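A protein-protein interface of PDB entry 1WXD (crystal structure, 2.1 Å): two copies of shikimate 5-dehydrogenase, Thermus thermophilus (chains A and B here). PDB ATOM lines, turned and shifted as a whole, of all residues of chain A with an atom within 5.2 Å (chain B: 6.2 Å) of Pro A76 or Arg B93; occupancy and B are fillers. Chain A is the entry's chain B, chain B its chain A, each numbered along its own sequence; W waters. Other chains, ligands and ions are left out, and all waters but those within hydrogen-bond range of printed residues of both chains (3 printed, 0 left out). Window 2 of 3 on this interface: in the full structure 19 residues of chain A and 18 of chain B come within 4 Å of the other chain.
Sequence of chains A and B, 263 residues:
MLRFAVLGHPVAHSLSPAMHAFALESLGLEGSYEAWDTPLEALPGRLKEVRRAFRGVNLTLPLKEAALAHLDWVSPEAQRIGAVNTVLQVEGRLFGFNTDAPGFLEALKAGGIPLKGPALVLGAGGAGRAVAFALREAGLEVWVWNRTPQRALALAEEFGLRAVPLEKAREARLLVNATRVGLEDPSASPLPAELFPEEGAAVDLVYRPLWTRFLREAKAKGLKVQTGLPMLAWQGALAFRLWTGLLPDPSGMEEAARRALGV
NH2 of Arg B93 is in salt-bridge range of OE1 of Glu A77 (3.1 Å).
O of Phe B95 lies within hydrogen-bond range of N of Leu B88.
The backbone NH of Glu B91 is in hydrogen-bond range of the side-chain amide oxygen of Gln B89.
Trp A73 touches Arg B93.
CZ of Phe B95 touches CZ3 of Trp A73, 3.5 Å away.
Arg B93 touches Pro A76.
Phe A97 touches Val B90 (CE2 to CG1, 3.4 Å).
CD2 of Phe A97 touches OE2 of Glu B91, 3.5 Å away.
Of chain B, only Arg B93 comes within 4 Å of Pro A76.
Of the printed residues of chain B, Glu A77 touches Arg B93 (3.1 Å).
Gln B89 touches none of the printed residues of chain A.
Of the printed residues of chain A, Val B90 touches Phe A97.
Of the printed residues of chain A, Glu B91 touches Phe A97 (3.5 Å).
Arg B93 touches just these residues of chain A: Trp A73 (3.8 Å), Pro A76 (3.7 Å) and Glu A77 (3.1 Å).
The nearest printed residue of chain A that does not touch Arg B93 is Phe A97 (5.2 Å).
Of the 10 printed residues of chain B, 4 touch a printed residue of chain A.
Of the 10 printed residues of chain A, 4 touch a printed residue of chain B.
Printed residues of chain A that touch a printed residue of chain B: Trp A73, Pro A76, Glu A77 and Phe A97.
Among the printed residues, 6 pairs touch across the chains.
Among the printed residues, Asp or Glu carboxylates within 4 Å of a Lys or Arg side-chain nitrogen of the other chain: Glu A77 with Arg B93.
No position is printed for both chains.
Of the 6 pairs that touch across the chains among the printed residues, none has its exchanged pair printed and touching as well.
Water W2 lies within hydrogen-bond range of OE1 of Glu A77 (2.6 Å), NE of Arg B93 (2.8 Å) and OE2 of Glu B91 (2.9 Å).
Water W1 lies within hydrogen-bond range of the side-chain carboxylate of Glu A77 (2.6 Å), the backbone carbonyl oxygen of Glu B91 (2.8 Å) and the guanidinium group of Arg B93 (3.0 Å).
Water W3 lies within hydrogen-bond range of the side-chain carboxylate (OE2) of Glu B91 (2.6 Å) and the side-chain hydroxyl (OG) of Ser A75 (2.7 Å).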
ATOM      1  N   TRP A  73     -11.732  -5.747  -2.354  1.00  0.00           N
ATOM      2  CA  TRP A  73     -12.160  -7.111  -2.060  1.00  0.00           C
ATOM      3  C   TRP A  73     -11.259  -7.707  -0.986  1.00  0.00           C
ATOM      4  O   TRP A  73     -10.039  -7.563  -1.043  1.00  0.00           O
ATOM      5  CB  TRP A  73     -12.078  -7.979  -3.315  1.00  0.00           C
ATOM      6  CG  TRP A  73     -12.551  -9.390  -3.114  1.00  0.00           C
ATOM      7  CD1 TRP A  73     -13.816  -9.865  -3.305  1.00  0.00           C
ATOM      8  CD2 TRP A  73     -11.762 -10.512  -2.694  1.00  0.00           C
ATOM      9  NE1 TRP A  73     -13.864 -11.213  -3.035  1.00  0.00           N
ATOM     10  CE2 TRP A  73     -12.617 -11.636  -2.657  1.00  0.00           C
ATOM     11  CE3 TRP A  73     -10.414 -10.678  -2.342  1.00  0.00           C
ATOM     12  CZ2 TRP A  73     -12.167 -12.912  -2.287  1.00  0.00           C
ATOM     13  CZ3 TRP A  73      -9.966 -11.948  -1.973  1.00  0.00           C
ATOM     14  CH2 TRP A  73     -10.842 -13.046  -1.950  1.00  0.00           C
ATOM     15  N   VAL A  74     -11.866  -8.377  -0.013  1.00  0.00           N
ATOM     16  CA  VAL A  74     -11.125  -9.003   1.077  1.00  0.00           C
ATOM     17  C   VAL A  74     -11.506 -10.480   1.140  1.00  0.00           C
ATOM     18  O   VAL A  74     -12.680 -10.828   1.028  1.00  0.00           O
ATOM     19  CB  VAL A  74     -11.454  -8.334   2.433  1.00  0.00           C
ATOM     20  CG1 VAL A  74     -10.577  -8.919   3.530  1.00  0.00           C
ATOM     21  CG2 VAL A  74     -11.251  -6.825   2.333  1.00  0.00           C
ATOM     22  N   SER A  75     -10.516 -11.346   1.316  1.00  0.00           N
ATOM     23  CA  SER A  75     -10.776 -12.779   1.373  1.00  0.00           C
ATOM     24  C   SER A  75     -11.657 -13.135   2.566  1.00  0.00           C
ATOM     25  O   SER A  75     -11.657 -12.436   3.581  1.00  0.00           O
ATOM     26  CB  SER A  75      -9.462 -13.566   1.463  1.00  0.00           C
ATOM     27  OG  SER A  75      -8.892 -13.469   2.761  1.00  0.00           O
ATOM     28  N   PRO A  76     -12.429 -14.227   2.450  1.00  0.00           N
ATOM     29  CA  PRO A  76     -13.312 -14.668   3.533  1.00  0.00           C
ATOM     30  C   PRO A  76     -12.482 -14.885   4.791  1.00  0.00           C
ATOM     31  O   PRO A  76     -12.851 -14.443   5.880  1.00  0.00           O
ATOM     32  CB  PRO A  76     -13.892 -15.972   2.993  1.00  0.00           C
ATOM     33  CG  PRO A  76     -13.939 -15.721   1.517  1.00  0.00           C
ATOM     34  CD  PRO A  76     -12.594 -15.082   1.262  1.00  0.00           C
ATOM     35  N   GLU A  77     -11.348 -15.561   4.626  1.00  0.00           N
ATOM     36  CA  GLU A  77     -10.454 -15.832   5.743  1.00  0.00           C
ATOM     37  C   GLU A  77      -9.997 -14.515   6.367  1.00  0.00           C
ATOM     38  O   GLU A  77     -10.050 -14.341   7.586  1.00  0.00           O
ATOM     39  CB  GLU A  77      -9.237 -16.640   5.274  1.00  0.00           C
ATOM     40  CG  GLU A  77      -9.575 -17.984   4.634  1.00  0.00           C
ATOM     41  CD  GLU A  77      -9.587 -17.930   3.113  1.00  0.00           C
ATOM     42  OE1 GLU A  77     -10.161 -16.971   2.554  1.00  0.00           O
ATOM     43  OE2 GLU A  77      -9.033 -18.856   2.476  1.00  0.00           O
ATOM     44  N   ALA A  78      -9.559 -13.581   5.529  1.00  0.00           N
ATOM     45  CA  ALA A  78      -9.102 -12.289   6.021  1.00  0.00           C
ATOM     46  C   ALA A  78     -10.246 -11.511   6.674  1.00  0.00           C
ATOM     47  O   ALA A  78     -10.021 -10.697   7.572  1.00  0.00           O
ATOM     48  CB  ALA A  78      -8.492 -11.478   4.882  1.00  0.00           C
ATOM     49  N   GLN A  79     -11.472 -11.755   6.224  1.00  0.00           N
ATOM     50  CA  GLN A  79     -12.616 -11.054   6.799  1.00  0.00           C
ATOM     51  C   GLN A  79     -12.912 -11.558   8.201  1.00  0.00           C
ATOM     52  O   GLN A  79     -13.154 -10.767   9.112  1.00  0.00           O
ATOM     53  CB  GLN A  79     -13.860 -11.219   5.927  1.00  0.00           C
ATOM     54  CG  GLN A  79     -13.761 -10.542   4.570  1.00  0.00           C
ATOM     55  CD  GLN A  79     -15.119 -10.308   3.938  1.00  0.00           C
ATOM     56  OE1 GLN A  79     -15.925  -9.533   4.450  1.00  0.00           O
ATOM     57  NE2 GLN A  79     -15.381 -10.982   2.822  1.00  0.00           N
ATOM     58  N   ARG A  80     -12.896 -12.874   8.376  1.00  0.00           N
ATOM     59  CA  ARG A  80     -13.162 -13.459   9.685  1.00  0.00           C
ATOM     60  C   ARG A  80     -12.065 -13.045  10.661  1.00  0.00           C
ATOM     61  O   ARG A  80     -12.339 -12.436  11.694  1.00  0.00           O
ATOM     62  CB  ARG A  80     -13.240 -14.983   9.584  1.00  0.00           C
ATOM     63  CG  ARG A  80     -13.504 -15.672  10.913  1.00  0.00           C
ATOM     64  CD  ARG A  80     -14.417 -16.880  10.744  1.00  0.00           C
ATOM     65  NE  ARG A  80     -15.752 -16.495  10.286  1.00  0.00           N
ATOM     66  CZ  ARG A  80     -16.587 -15.716  10.970  1.00  0.00           C
ATOM     67  NH1 ARG A  80     -16.235 -15.230  12.153  1.00  0.00           N
ATOM     68  NH2 ARG A  80     -17.778 -15.421  10.471  1.00  0.00           N
ATOM     69  N   ILE A  81     -10.822 -13.371  10.324  1.00  0.00           N
ATOM     70  CA  ILE A  81      -9.688 -13.010  11.166  1.00  0.00           C
ATOM     71  C   ILE A  81      -9.751 -11.520  11.473  1.00  0.00           C
ATOM     72  O   ILE A  81      -9.450 -11.090  12.589  1.00  0.00           O
ATOM     73  CB  ILE A  81      -8.349 -13.311  10.461  1.00  0.00           C
ATOM     74  CG1 ILE A  81      -8.202 -14.820  10.257  1.00  0.00           C
ATOM     75  CG2 ILE A  81      -7.188 -12.755  11.281  1.00  0.00           C
ATOM     76  CD1 ILE A  81      -6.985 -15.220   9.441  1.00  0.00           C
ATOM     77  N   PHE A  97      -5.669 -10.217   1.397  1.00  0.00           N
ATOM     78  CA  PHE A  97      -5.613 -11.607   1.831  1.00  0.00           C
ATOM     79  C   PHE A  97      -4.850 -11.719   3.153  1.00  0.00           C
ATOM     80  O   PHE A  97      -4.251 -10.750   3.629  1.00  0.00           O
ATOM     81  CB  PHE A  97      -4.905 -12.477   0.787  1.00  0.00           C
ATOM     82  CG  PHE A  97      -5.432 -12.319  -0.613  1.00  0.00           C
ATOM     83  CD1 PHE A  97      -5.069 -11.224  -1.391  1.00  0.00           C
ATOM     84  CD2 PHE A  97      -6.271 -13.281  -1.163  1.00  0.00           C
ATOM     85  CE1 PHE A  97      -5.530 -11.093  -2.696  1.00  0.00           C
ATOM     86  CE2 PHE A  97      -6.742 -13.158  -2.472  1.00  0.00           C
ATOM     87  CZ  PHE A  97      -6.366 -12.061  -3.236  1.00  0.00           C
ATOM     88  N   ARG B  51      -9.634 -23.530 -10.071  1.00  0.00           N
ATOM     89  CA  ARG B  51      -9.333 -23.100  -8.700  1.00  0.00           C
ATOM     90  C   ARG B  51      -8.266 -23.975  -8.017  1.00  0.00           C
ATOM     91  O   ARG B  51      -7.549 -23.542  -7.125  1.00  0.00           O
ATOM     92  CB  ARG B  51     -10.633 -23.136  -7.893  1.00  0.00           C
ATOM     93  CG  ARG B  51     -11.553 -21.959  -8.221  1.00  0.00           C
ATOM     94  CD  ARG B  51     -12.847 -21.990  -7.399  1.00  0.00           C
ATOM     95  NE  ARG B  51     -13.619 -20.762  -7.608  1.00  0.00           N
ATOM     96  CZ  ARG B  51     -14.827 -20.682  -7.019  1.00  0.00           C
ATOM     97  NH1 ARG B  51     -15.275 -21.683  -6.284  1.00  0.00           N
ATOM     98  NH2 ARG B  51     -15.568 -19.581  -7.180  1.00  0.00           N
ATOM     99  N   ASP B  72     -15.868 -15.114  -7.917  1.00  0.00           N
ATOM    100  CA  ASP B  72     -15.899 -14.474  -6.606  1.00  0.00           C
ATOM    101  C   ASP B  72     -15.953 -12.958  -6.713  1.00  0.00           C
ATOM    102  O   ASP B  72     -16.518 -12.283  -5.854  1.00  0.00           O
ATOM    103  CB  ASP B  72     -14.664 -14.874  -5.799  1.00  0.00           C
ATOM    104  CG  ASP B  72     -14.631 -16.351  -5.485  1.00  0.00           C
ATOM    105  OD1 ASP B  72     -15.529 -16.818  -4.753  1.00  0.00           O
ATOM    106  OD2 ASP B  72     -13.715 -17.046  -5.970  1.00  0.00           O
ATOM    107  N   LEU B  88      -8.386 -14.866 -13.038  1.00  0.00           N
ATOM    108  CA  LEU B  88      -7.193 -15.036 -12.212  1.00  0.00           C
ATOM    109  C   LEU B  88      -7.548 -15.871 -10.987  1.00  0.00           C
ATOM    110  O   LEU B  88      -8.555 -15.607 -10.328  1.00  0.00           O
ATOM    111  CB  LEU B  88      -6.665 -13.679 -11.741  1.00  0.00           C
ATOM    112  CG  LEU B  88      -5.675 -13.715 -10.568  1.00  0.00           C
ATOM    113  CD1 LEU B  88      -4.321 -14.250 -11.037  1.00  0.00           C
ATOM    114  CD2 LEU B  88      -5.516 -12.318 -10.000  1.00  0.00           C
ATOM    115  N   GLN B  89      -6.729 -16.876 -10.691  1.00  0.00           N
ATOM    116  CA  GLN B  89      -6.959 -17.717  -9.525  1.00  0.00           C
ATOM    117  C   GLN B  89      -5.902 -17.442  -8.468  1.00  0.00           C
ATOM    118  O   GLN B  89      -4.700 -17.506  -8.736  1.00  0.00           O
ATOM    119  CB  GLN B  89      -6.935 -19.203  -9.907  1.00  0.00           C
ATOM    120  CG  GLN B  89      -7.151 -20.169  -8.735  1.00  0.00           C
ATOM    121  CD  GLN B  89      -5.893 -20.407  -7.908  1.00  0.00           C
ATOM    122  OE1 GLN B  89      -5.793 -19.962  -6.761  1.00  0.00           O
ATOM    123  NE2 GLN B  89      -4.926 -21.114  -8.486  1.00  0.00           N
ATOM    124  N   VAL B  90      -6.367 -17.109  -7.271  1.00  0.00           N
ATOM    125  CA  VAL B  90      -5.505 -16.836  -6.127  1.00  0.00           C
ATOM    126  C   VAL B  90      -6.190 -17.439  -4.902  1.00  0.00           C
ATOM    127  O   VAL B  90      -7.370 -17.195  -4.658  1.00  0.00           O
ATOM    128  CB  VAL B  90      -5.309 -15.314  -5.910  1.00  0.00           C
ATOM    129  CG1 VAL B  90      -4.763 -15.065  -4.520  1.00  0.00           C
ATOM    130  CG2 VAL B  90      -4.345 -14.764  -6.949  1.00  0.00           C
ATOM    131  N   GLU B  91      -5.444 -18.224  -4.138  1.00  0.00           N
ATOM    132  CA  GLU B  91      -5.987 -18.877  -2.954  1.00  0.00           C
ATOM    133  C   GLU B  91      -7.313 -19.563  -3.247  1.00  0.00           C
ATOM    134  O   GLU B  91      -8.194 -19.614  -2.394  1.00  0.00           O
ATOM    135  CB  GLU B  91      -6.171 -17.878  -1.811  1.00  0.00           C
ATOM    136  CG  GLU B  91      -4.895 -17.579  -1.058  1.00  0.00           C
ATOM    137  CD  GLU B  91      -5.128 -16.747   0.192  1.00  0.00           C
ATOM    138  OE1 GLU B  91      -4.143 -16.489   0.917  1.00  0.00           O
ATOM    139  OE2 GLU B  91      -6.286 -16.348   0.451  1.00  0.00           O
ATOM    140  N   GLY B  92      -7.452 -20.083  -4.464  1.00  0.00           N
ATOM    141  CA  GLY B  92      -8.677 -20.769  -4.830  1.00  0.00           C
ATOM    142  C   GLY B  92      -9.832 -19.866  -5.215  1.00  0.00           C
ATOM    143  O   GLY B  92     -10.877 -20.355  -5.637  1.00  0.00           O
ATOM    144  N   ARG B  93      -9.663 -18.555  -5.063  1.00  0.00           N
ATOM    145  CA  ARG B  93     -10.720 -17.613  -5.432  1.00  0.00           C
ATOM    146  C   ARG B  93     -10.535 -17.232  -6.902  1.00  0.00           C
ATOM    147  O   ARG B  93      -9.407 -17.215  -7.406  1.00  0.00           O
ATOM    148  CB  ARG B  93     -10.647 -16.358  -4.561  1.00  0.00           C
ATOM    149  CG  ARG B  93     -10.489 -16.644  -3.081  1.00  0.00           C
ATOM    150  CD  ARG B  93     -11.654 -17.452  -2.543  1.00  0.00           C
ATOM    151  NE  ARG B  93     -11.424 -17.857  -1.160  1.00  0.00           N
ATOM    152  CZ  ARG B  93     -12.315 -18.495  -0.407  1.00  0.00           C
ATOM    153  NH1 ARG B  93     -13.507 -18.806  -0.901  1.00  0.00           N
ATOM    154  NH2 ARG B  93     -12.016 -18.815   0.844  1.00  0.00           N
ATOM    155  N   LEU B  94     -11.639 -16.928  -7.581  1.00  0.00           N
ATOM    156  CA  LEU B  94     -11.603 -16.561  -8.996  1.00  0.00           C
ATOM    157  C   LEU B  94     -12.037 -15.121  -9.232  1.00  0.00           C
ATOM    158  O   LEU B  94     -13.104 -14.700  -8.780  1.00  0.00           O
ATOM    159  CB  LEU B  94     -12.501 -17.499  -9.805  1.00  0.00           C
ATOM    160  CG  LEU B  94     -12.132 -18.982  -9.726  1.00  0.00           C
ATOM    161  CD1 LEU B  94     -13.086 -19.793 -10.596  1.00  0.00           C
ATOM    162  CD2 LEU B  94     -10.686 -19.173 -10.178  1.00  0.00           C
ATOM    163  N   PHE B  95     -11.208 -14.375  -9.954  1.00  0.00           N
ATOM    164  CA  PHE B  95     -11.491 -12.976 -10.252  1.00  0.00           C
ATOM    165  C   PHE B  95     -11.597 -12.796 -11.762  1.00  0.00           C
ATOM    166  O   PHE B  95     -10.730 -13.260 -12.511  1.00  0.00           O
ATOM    167  CB  PHE B  95     -10.372 -12.099  -9.684  1.00  0.00           C
ATOM    168  CG  PHE B  95     -10.207 -12.221  -8.194  1.00  0.00           C
ATOM    169  CD1 PHE B  95     -10.791 -11.296  -7.335  1.00  0.00           C
ATOM    170  CD2 PHE B  95      -9.497 -13.283  -7.646  1.00  0.00           C
ATOM    171  CE1 PHE B  95     -10.673 -11.431  -5.948  1.00  0.00           C
ATOM    172  CE2 PHE B  95      -9.374 -13.426  -6.262  1.00  0.00           C
ATOM    173  CZ  PHE B  95      -9.964 -12.498  -5.414  1.00  0.00           C
HETATM  174  O   HOH W   1      -9.315 -19.968   0.131  1.00  0.00           O
HETATM  175  O   HOH W   2      -9.141 -16.868   0.175  1.00  0.00           O
HETATM  176  O   HOH W   3      -6.608 -14.903   2.643  1.00  0.00           O
